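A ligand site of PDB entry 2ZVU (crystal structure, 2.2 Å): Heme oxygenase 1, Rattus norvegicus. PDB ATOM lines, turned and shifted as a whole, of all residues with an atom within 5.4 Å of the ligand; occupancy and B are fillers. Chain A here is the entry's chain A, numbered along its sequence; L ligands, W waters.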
ATOM      1  N   SER A  14     -11.811  16.737 -19.893  1.00  0.00           N
ATOM      2  CA  SER A  14     -12.867  17.643 -19.400  1.00  0.00           C
ATOM      3  C   SER A  14     -12.333  19.069 -19.247  1.00  0.00           C
ATOM      4  O   SER A  14     -13.022  20.032 -19.593  1.00  0.00           O
ATOM      5  CB  SER A  14     -13.417  17.145 -18.061  1.00  0.00           C
ATOM      6  OG  SER A  14     -12.408  17.179 -17.038  1.00  0.00           O
ATOM      7  N   LEU A  17     -11.283  20.488 -22.793  1.00  0.00           N
ATOM      8  CA  LEU A  17     -12.471  20.972 -23.492  1.00  0.00           C
ATOM      9  C   LEU A  17     -12.984  22.322 -22.960  1.00  0.00           C
ATOM     10  O   LEU A  17     -13.408  23.179 -23.741  1.00  0.00           O
ATOM     11  CB  LEU A  17     -13.565  19.924 -23.451  1.00  0.00           C
ATOM     12  CG  LEU A  17     -13.469  18.861 -24.543  1.00  0.00           C
ATOM     13  CD1 LEU A  17     -14.482  17.772 -24.295  1.00  0.00           C
ATOM     14  CD2 LEU A  17     -13.723  19.500 -25.878  1.00  0.00           C
ATOM     15  N   LYS A  18     -12.955  22.505 -21.645  1.00  0.00           N
ATOM     16  CA  LYS A  18     -13.400  23.780 -21.062  1.00  0.00           C
ATOM     17  C   LYS A  18     -12.472  24.924 -21.484  1.00  0.00           C
ATOM     18  O   LYS A  18     -12.925  25.977 -21.925  1.00  0.00           O
ATOM     19  CB  LYS A  18     -13.497  23.701 -19.545  1.00  0.00           C
ATOM     20  CG  LYS A  18     -14.434  24.741 -18.973  1.00  0.00           C
ATOM     21  CD  LYS A  18     -14.166  25.017 -17.529  1.00  0.00           C
ATOM     22  CE  LYS A  18     -15.023  26.188 -17.056  1.00  0.00           C
ATOM     23  NZ  LYS A  18     -15.230  26.191 -15.575  1.00  0.00           N
ATOM     24  N   HIS A  25     -17.249  30.287 -26.118  1.00  0.00           N
ATOM     25  CA  HIS A  25     -18.440  30.263 -25.262  1.00  0.00           C
ATOM     26  C   HIS A  25     -18.897  31.691 -24.950  1.00  0.00           C
ATOM     27  O   HIS A  25     -20.093  32.011 -25.001  1.00  0.00           O
ATOM     28  CB  HIS A  25     -18.206  29.491 -23.963  1.00  0.00           C
ATOM     29  CG  HIS A  25     -19.436  29.434 -23.125  1.00  0.00           C
ATOM     30  ND1 HIS A  25     -19.796  30.463 -22.270  1.00  0.00           N
ATOM     31  CD2 HIS A  25     -20.452  28.540 -23.085  1.00  0.00           C
ATOM     32  CE1 HIS A  25     -20.955  30.165 -21.705  1.00  0.00           C
ATOM     33  NE2 HIS A  25     -21.370  29.009 -22.175  1.00  0.00           N
ATOM     34  N   ALA A  28     -20.630  33.009 -27.942  1.00  0.00           N
ATOM     35  CA  ALA A  28     -21.927  32.339 -28.072  1.00  0.00           C
ATOM     36  C   ALA A  28     -22.969  32.897 -27.101  1.00  0.00           C
ATOM     37  O   ALA A  28     -24.069  33.195 -27.502  1.00  0.00           O
ATOM     38  CB  ALA A  28     -21.808  30.808 -27.917  1.00  0.00           C
ATOM     39  N   GLU A  29     -22.614  33.041 -25.829  1.00  0.00           N
ATOM     40  CA  GLU A  29     -23.591  33.552 -24.867  1.00  0.00           C
ATOM     41  C   GLU A  29     -23.913  35.022 -25.083  1.00  0.00           C
ATOM     42  O   GLU A  29     -24.879  35.538 -24.520  1.00  0.00           O
ATOM     43  CB  GLU A  29     -23.197  33.265 -23.415  1.00  0.00           C
ATOM     44  CG  GLU A  29     -21.998  34.007 -22.924  1.00  0.00           C
ATOM     45  CD  GLU A  29     -21.660  33.663 -21.491  1.00  0.00           C
ATOM     46  OE1 GLU A  29     -22.592  33.698 -20.646  1.00  0.00           O
ATOM     47  OE2 GLU A  29     -20.466  33.374 -21.228  1.00  0.00           O
ATOM     48  N   ASN A  30     -23.134  35.682 -25.935  1.00  0.00           N
ATOM     49  CA  ASN A  30     -23.318  37.091 -26.220  1.00  0.00           C
ATOM     50  C   ASN A  30     -23.734  37.331 -27.643  1.00  0.00           C
ATOM     51  O   ASN A  30     -23.679  38.460 -28.117  1.00  0.00           O
ATOM     52  CB  ASN A  30     -22.045  37.872 -25.915  1.00  0.00           C
ATOM     53  CG  ASN A  30     -21.830  38.064 -24.466  1.00  0.00           C
ATOM     54  OD1 ASN A  30     -22.581  38.766 -23.807  1.00  0.00           O
ATOM     55  ND2 ASN A  30     -20.784  37.441 -23.935  1.00  0.00           N
ATOM     56  N   MET A  34     -29.142  35.628 -28.452  1.00  0.00           N
ATOM     57  CA  MET A  34     -29.101  35.290 -27.032  1.00  0.00           C
ATOM     58  C   MET A  34     -29.191  36.505 -26.123  1.00  0.00           C
ATOM     59  O   MET A  34     -29.828  36.440 -25.070  1.00  0.00           O
ATOM     60  CB  MET A  34     -27.890  34.429 -26.690  1.00  0.00           C
ATOM     61  CG  MET A  34     -27.936  32.993 -27.238  1.00  0.00           C
ATOM     62  SD  MET A  34     -29.366  31.954 -26.766  1.00  0.00           S
ATOM     63  CE  MET A  34     -29.736  32.581 -25.146  1.00  0.00           C
ATOM     64  N   GLN A  38     -31.975  36.766 -23.374  1.00  0.00           N
ATOM     65  CA  GLN A  38     -31.666  37.064 -21.969  1.00  0.00           C
ATOM     66  C   GLN A  38     -32.312  38.326 -21.450  1.00  0.00           C
ATOM     67  O   GLN A  38     -32.581  38.435 -20.258  1.00  0.00           O
ATOM     68  CB  GLN A  38     -30.155  37.116 -21.757  1.00  0.00           C
ATOM     69  CG  GLN A  38     -29.523  35.756 -21.619  1.00  0.00           C
ATOM     70  CD  GLN A  38     -28.097  35.756 -22.089  1.00  0.00           C
ATOM     71  OE1 GLN A  38     -27.205  36.157 -21.353  1.00  0.00           O
ATOM     72  NE2 GLN A  38     -27.874  35.298 -23.313  1.00  0.00           N
ATOM     73  N   TYR A 134     -20.831  16.699 -25.605  1.00  0.00           N
ATOM     74  CA  TYR A 134     -20.333  17.705 -24.668  1.00  0.00           C
ATOM     75  C   TYR A 134     -20.963  19.079 -24.900  1.00  0.00           C
ATOM     76  O   TYR A 134     -21.588  19.643 -23.991  1.00  0.00           O
ATOM     77  CB  TYR A 134     -18.804  17.803 -24.743  1.00  0.00           C
ATOM     78  CG  TYR A 134     -18.205  19.003 -24.049  1.00  0.00           C
ATOM     79  CD1 TYR A 134     -17.978  19.001 -22.670  1.00  0.00           C
ATOM     80  CD2 TYR A 134     -17.832  20.143 -24.786  1.00  0.00           C
ATOM     81  CE1 TYR A 134     -17.402  20.121 -22.023  1.00  0.00           C
ATOM     82  CE2 TYR A 134     -17.265  21.256 -24.162  1.00  0.00           C
ATOM     83  CZ  TYR A 134     -17.049  21.239 -22.784  1.00  0.00           C
ATOM     84  OH  TYR A 134     -16.477  22.363 -22.195  1.00  0.00           O
ATOM     85  N   THR A 135     -20.837  19.610 -26.130  1.00  0.00           N
ATOM     86  CA  THR A 135     -21.240  20.982 -26.443  1.00  0.00           C
ATOM     87  C   THR A 135     -22.727  21.219 -26.179  1.00  0.00           C
ATOM     88  O   THR A 135     -23.124  22.287 -25.668  1.00  0.00           O
ATOM     89  CB  THR A 135     -20.859  21.347 -27.919  1.00  0.00           C
ATOM     90  OG1 THR A 135     -19.432  21.459 -28.052  1.00  0.00           O
ATOM     91  CG2 THR A 135     -21.566  22.661 -28.393  1.00  0.00           C
ATOM     92  N   ARG A 136     -23.573  20.252 -26.553  1.00  0.00           N
ATOM     93  CA  ARG A 136     -24.996  20.407 -26.337  1.00  0.00           C
ATOM     94  C   ARG A 136     -25.429  20.044 -24.905  1.00  0.00           C
ATOM     95  O   ARG A 136     -25.974  20.879 -24.205  1.00  0.00           O
ATOM     96  CB  ARG A 136     -25.812  19.650 -27.388  1.00  0.00           C
ATOM     97  CG  ARG A 136     -25.822  20.249 -28.807  1.00  0.00           C
ATOM     98  CD  ARG A 136     -26.362  21.715 -28.925  1.00  0.00           C
ATOM     99  NE  ARG A 136     -27.434  22.035 -27.970  1.00  0.00           N
ATOM    100  CZ  ARG A 136     -27.901  23.262 -27.731  1.00  0.00           C
ATOM    101  NH1 ARG A 136     -28.855  23.460 -26.836  1.00  0.00           N
ATOM    102  NH2 ARG A 136     -27.381  24.303 -28.361  1.00  0.00           N
ATOM    103  N   LEU A 138     -23.925  19.487 -21.872  1.00  0.00           N
ATOM    104  CA  LEU A 138     -23.407  20.159 -20.665  1.00  0.00           C
ATOM    105  C   LEU A 138     -23.875  21.603 -20.599  1.00  0.00           C
ATOM    106  O   LEU A 138     -23.989  22.172 -19.510  1.00  0.00           O
ATOM    107  CB  LEU A 138     -21.878  20.052 -20.560  1.00  0.00           C
ATOM    108  CG  LEU A 138     -21.254  18.690 -20.158  1.00  0.00           C
ATOM    109  CD1 LEU A 138     -20.115  18.914 -19.174  1.00  0.00           C
ATOM    110  CD2 LEU A 138     -22.274  17.682 -19.573  1.00  0.00           C
ATOM    111  N   GLY A 139     -24.130  22.201 -21.767  1.00  0.00           N
ATOM    112  CA  GLY A 139     -24.801  23.487 -21.804  1.00  0.00           C
ATOM    113  C   GLY A 139     -26.240  23.362 -21.385  1.00  0.00           C
ATOM    114  O   GLY A 139     -26.733  24.180 -20.598  1.00  0.00           O
ATOM    115  N   SER A 142     -26.547  23.583 -17.893  1.00  0.00           N
ATOM    116  CA  SER A 142     -25.937  24.778 -17.319  1.00  0.00           C
ATOM    117  C   SER A 142     -26.737  26.020 -17.637  1.00  0.00           C
ATOM    118  O   SER A 142     -27.713  26.315 -16.945  1.00  0.00           O
ATOM    119  CB  SER A 142     -24.517  24.946 -17.844  1.00  0.00           C
ATOM    120  OG  SER A 142     -23.802  23.758 -17.614  1.00  0.00           O
ATOM    121  N   GLY A 143     -26.331  26.737 -18.683  1.00  0.00           N
ATOM    122  CA  GLY A 143     -27.045  27.920 -19.163  1.00  0.00           C
ATOM    123  C   GLY A 143     -28.442  27.596 -19.662  1.00  0.00           C
ATOM    124  O   GLY A 143     -29.340  28.424 -19.542  1.00  0.00           O
ATOM    125  N   VAL A 146     -30.873  28.436 -17.077  1.00  0.00           N
ATOM    126  CA  VAL A 146     -31.133  29.864 -17.001  1.00  0.00           C
ATOM    127  C   VAL A 146     -32.060  30.283 -18.138  1.00  0.00           C
ATOM    128  O   VAL A 146     -33.026  31.008 -17.927  1.00  0.00           O
ATOM    129  CB  VAL A 146     -29.819  30.676 -17.051  1.00  0.00           C
ATOM    130  CG1 VAL A 146     -30.088  32.147 -16.951  1.00  0.00           C
ATOM    131  CG2 VAL A 146     -28.868  30.215 -15.922  1.00  0.00           C
ATOM    132  N   LEU A 147     -31.794  29.780 -19.346  1.00  0.00           N
ATOM    133  CA  LEU A 147     -32.672  30.051 -20.479  1.00  0.00           C
ATOM    134  C   LEU A 147     -34.107  29.630 -20.195  1.00  0.00           C
ATOM    135  O   LEU A 147     -35.053  30.323 -20.566  1.00  0.00           O
ATOM    136  CB  LEU A 147     -32.148  29.375 -21.752  1.00  0.00           C
ATOM    137  CG  LEU A 147     -30.790  29.874 -22.302  1.00  0.00           C
ATOM    138  CD1 LEU A 147     -30.383  29.070 -23.504  1.00  0.00           C
ATOM    139  CD2 LEU A 147     -30.864  31.341 -22.661  1.00  0.00           C
ATOM    140  N   LYS A 179     -23.127  16.674 -14.073  1.00  0.00           N
ATOM    141  CA  LYS A 179     -22.039  17.266 -14.848  1.00  0.00           C
ATOM    142  C   LYS A 179     -20.667  16.815 -14.326  1.00  0.00           C
ATOM    143  O   LYS A 179     -19.765  16.515 -15.113  1.00  0.00           O
ATOM    144  CB  LYS A 179     -22.131  18.798 -14.871  1.00  0.00           C
ATOM    145  CG  LYS A 179     -22.941  19.355 -16.036  1.00  0.00           C
ATOM    146  CD  LYS A 179     -22.938  20.878 -16.030  1.00  0.00           C
ATOM    147  CE  LYS A 179     -23.642  21.427 -14.774  1.00  0.00           C
ATOM    148  NZ  LYS A 179     -23.336  22.856 -14.539  1.00  0.00           N
ATOM    149  N   ARG A 183     -18.129  14.695 -16.561  1.00  0.00           N
ATOM    150  CA  ARG A 183     -16.751  15.129 -16.731  1.00  0.00           C
ATOM    151  C   ARG A 183     -15.754  14.028 -16.388  1.00  0.00           C
ATOM    152  O   ARG A 183     -14.885  13.716 -17.187  1.00  0.00           O
ATOM    153  CB  ARG A 183     -16.453  16.398 -15.921  1.00  0.00           C
ATOM    154  CG  ARG A 183     -17.028  17.681 -16.510  1.00  0.00           C
ATOM    155  CD  ARG A 183     -16.533  18.879 -15.695  1.00  0.00           C
ATOM    156  NE  ARG A 183     -17.315  20.069 -15.985  1.00  0.00           N
ATOM    157  CZ  ARG A 183     -18.272  20.583 -15.206  1.00  0.00           C
ATOM    158  NH1 ARG A 183     -18.585  19.993 -14.056  1.00  0.00           N
ATOM    159  NH2 ARG A 183     -18.927  21.670 -15.578  1.00  0.00           N
ATOM    160  N   PHE A 207     -19.492  24.711 -31.338  1.00  0.00           N
ATOM    161  CA  PHE A 207     -19.891  26.042 -30.867  1.00  0.00           C
ATOM    162  C   PHE A 207     -20.202  26.977 -32.024  1.00  0.00           C
ATOM    163  O   PHE A 207     -21.165  27.730 -31.951  1.00  0.00           O
ATOM    164  CB  PHE A 207     -18.848  26.686 -29.948  1.00  0.00           C
ATOM    165  CG  PHE A 207     -19.058  26.382 -28.481  1.00  0.00           C
ATOM    166  CD1 PHE A 207     -18.469  25.250 -27.893  1.00  0.00           C
ATOM    167  CD2 PHE A 207     -19.837  27.212 -27.685  1.00  0.00           C
ATOM    168  CE1 PHE A 207     -18.662  24.962 -26.539  1.00  0.00           C
ATOM    169  CE2 PHE A 207     -20.036  26.941 -26.333  1.00  0.00           C
ATOM    170  CZ  PHE A 207     -19.445  25.808 -25.760  1.00  0.00           C
ATOM    171  N   ASN A 210     -23.517  26.321 -33.618  1.00  0.00           N
ATOM    172  CA  ASN A 210     -24.540  26.931 -32.770  1.00  0.00           C
ATOM    173  C   ASN A 210     -24.585  28.446 -32.964  1.00  0.00           C
ATOM    174  O   ASN A 210     -25.644  29.003 -33.133  1.00  0.00           O
ATOM    175  CB  ASN A 210     -24.304  26.610 -31.281  1.00  0.00           C
ATOM    176  CG  ASN A 210     -24.815  25.235 -30.904  1.00  0.00           C
ATOM    177  OD1 ASN A 210     -26.005  25.045 -30.681  1.00  0.00           O
ATOM    178  ND2 ASN A 210     -23.927  24.275 -30.880  1.00  0.00           N
ATOM    179  N   PHE A 214     -27.821  30.531 -34.478  1.00  0.00           N
ATOM    180  CA  PHE A 214     -28.431  31.687 -33.817  1.00  0.00           C
ATOM    181  C   PHE A 214     -28.348  32.968 -34.635  1.00  0.00           C
ATOM    182  O   PHE A 214     -29.281  33.749 -34.603  1.00  0.00           O
ATOM    183  CB  PHE A 214     -27.893  31.891 -32.387  1.00  0.00           C
ATOM    184  CG  PHE A 214     -28.192  30.741 -31.474  1.00  0.00           C
ATOM    185  CD1 PHE A 214     -29.481  30.243 -31.358  1.00  0.00           C
ATOM    186  CD2 PHE A 214     -27.182  30.150 -30.722  1.00  0.00           C
ATOM    187  CE1 PHE A 214     -29.761  29.168 -30.533  1.00  0.00           C
ATOM    188  CE2 PHE A 214     -27.453  29.081 -29.875  1.00  0.00           C
ATOM    189  CZ  PHE A 214     -28.739  28.581 -29.786  1.00  0.00           C
HETATM  190  O1  LIG L   1     -17.855  23.015 -17.748  1.00  0.00           O
HETATM  191  C1  LIG L   1     -17.676  23.049 -18.986  1.00  0.00           C
HETATM  192  O2  LIG L   1     -16.807  22.343 -19.541  1.00  0.00           O
HETATM  193  C2  LIG L   1     -18.515  24.012 -19.791  1.00  0.00           C
HETATM  194  C3  LIG L   1     -19.997  23.603 -19.994  1.00  0.00           C
HETATM  195  C4  LIG L   1     -20.511  24.574 -21.069  1.00  0.00           C
HETATM  196  C5  LIG L   1     -21.338  24.001 -22.191  1.00  0.00           C
HETATM  197  C6  LIG L   1     -20.529  23.207 -23.222  1.00  0.00           C
HETATM  198  C7  LIG L   1     -21.344  25.752 -20.642  1.00  0.00           C
HETATM  199  C8  LIG L   1     -21.263  26.285 -19.408  1.00  0.00           C
HETATM  200  N1  LIG L   1     -22.092  26.198 -21.683  1.00  0.00           N
HETATM  201  C9  LIG L   1     -22.009  25.265 -22.671  1.00  0.00           C
HETATM  202  C10 LIG L   1     -22.438  25.410 -23.932  1.00  0.00           C
HETATM  203  C11 LIG L   1     -23.174  26.551 -24.506  1.00  0.00           C
HETATM  204  C12 LIG L   1     -23.618  26.723 -25.906  1.00  0.00           C
HETATM  205  C13 LIG L   1     -23.361  25.728 -26.972  1.00  0.00           C
HETATM  206  C14 LIG L   1     -24.364  25.207 -27.637  1.00  0.00           C
HETATM  207  C15 LIG L   1     -24.271  27.961 -25.988  1.00  0.00           C
HETATM  208  C16 LIG L   1     -24.915  28.609 -27.208  1.00  0.00           C
HETATM  209 FE1  LIG L   1     -23.091  27.801 -21.762  1.00  0.00          FE
HETATM  210  N2  LIG L   1     -22.862  28.099 -19.717  1.00  0.00           N
HETATM  211  C17 LIG L   1     -22.080  27.412 -18.890  1.00  0.00           C
HETATM  212  N3  LIG L   1     -23.511  27.591 -23.769  1.00  0.00           N
HETATM  213  C18 LIG L   1     -24.158  28.452 -24.582  1.00  0.00           C
HETATM  214  O3  LIG L   1     -24.668  29.583 -24.249  1.00  0.00           O
HETATM  215  C19 LIG L   1     -24.867  29.974 -23.031  1.00  0.00           C
HETATM  216  C20 LIG L   1     -25.745  31.127 -22.702  1.00  0.00           C
HETATM  217  C21 LIG L   1     -26.515  31.995 -23.626  1.00  0.00           C
HETATM  218  C22 LIG L   1     -26.515  31.727 -24.910  1.00  0.00           C
HETATM  219  C23 LIG L   1     -25.724  31.314 -21.330  1.00  0.00           C
HETATM  220  C24 LIG L   1     -26.442  32.358 -20.498  1.00  0.00           C
HETATM  221  N4  LIG L   1     -24.320  29.474 -21.900  1.00  0.00           N
HETATM  222  C25 LIG L   1     -24.810  30.234 -20.893  1.00  0.00           C
HETATM  223  C26 LIG L   1     -24.445  29.994 -19.478  1.00  0.00           C
HETATM  224  C27 LIG L   1     -23.449  29.024 -18.951  1.00  0.00           C
HETATM  225  C28 LIG L   1     -23.032  28.932 -17.524  1.00  0.00           C
HETATM  226  C29 LIG L   1     -23.515  29.806 -16.395  1.00  0.00           C
HETATM  227  C30 LIG L   1     -22.126  27.882 -17.476  1.00  0.00           C
HETATM  228  C31 LIG L   1     -21.392  27.330 -16.265  1.00  0.00           C
HETATM  229  C32 LIG L   1     -19.960  27.852 -16.155  1.00  0.00           C
HETATM  230  C33 LIG L   1     -19.307  27.380 -14.861  1.00  0.00           C
HETATM  231  O4  LIG L   1     -19.016  26.159 -14.724  1.00  0.00           O
HETATM  232  O5  LIG L   1     -19.061  28.238 -13.970  1.00  0.00           O
HETATM  233  O   HOH W   1     -25.601  26.706 -21.935  1.00  0.00           O
HETATM  234  O   HOH W   2     -27.938  27.019 -26.545  1.00  0.00           O
HETATM  235  O   HOH W   3     -25.735  23.659 -25.065  1.00  0.00           O
HETATM  236  O   HOH W   4     -15.196  20.530 -18.386  1.00  0.00           O
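Water W4 lies within hydrogen-bond range of O of Ser 14 (2.5 Å), O2 of the ligand (2.7 Å) and NE of Arg 183 (3.2 Å).
Residues that only touch the ligand: Met 34, Arg 136, Asn 210, Gly 143, Gly 139, Glu 29, Phe 207, Gln 38, Ser 142, Thr 135, Phe 214, Leu 138 and Ala 28.
FE1 of the ligand is bound by NE2 of His 25 (2.1 Å).
The side-chain hydroxyl (OH) of Tyr 134 lies within hydrogen-bond range of an oxygen (O2) of the ligand (2.7 Å).
NH2 of Arg 183 is in salt-bridge range of O1 of the ligand, 2.8 Å away.
NZ of Lys 18 lies within salt-bridge range of O4 of the ligand, 3.9 Å away.
OE2 of Glu 29 sits at hydrogen-bond distance from ND1 of His 25.
O of Met 34 is in hydrogen-bond range of NE2 of Gln 38.
The guanidinium group of Arg 136 sits at hydrogen-bond distance from the side-chain amide oxygen of Asn 210 (2.8 Å).
NE2 of Gln 38 sits at hydrogen-bond distance from O of Glu 29 (3.2 Å).
The side-chain hydroxyl (OG) of Ser 142 is in hydrogen-bond range of the backbone carbonyl oxygen (O) of Leu 138, at 2.5 Å.
The side-chain hydroxyl (OG) of Ser 142 lies within hydrogen-bond range of the side-chain amino group (NZ) of Lys 179, 3.2 Å away.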
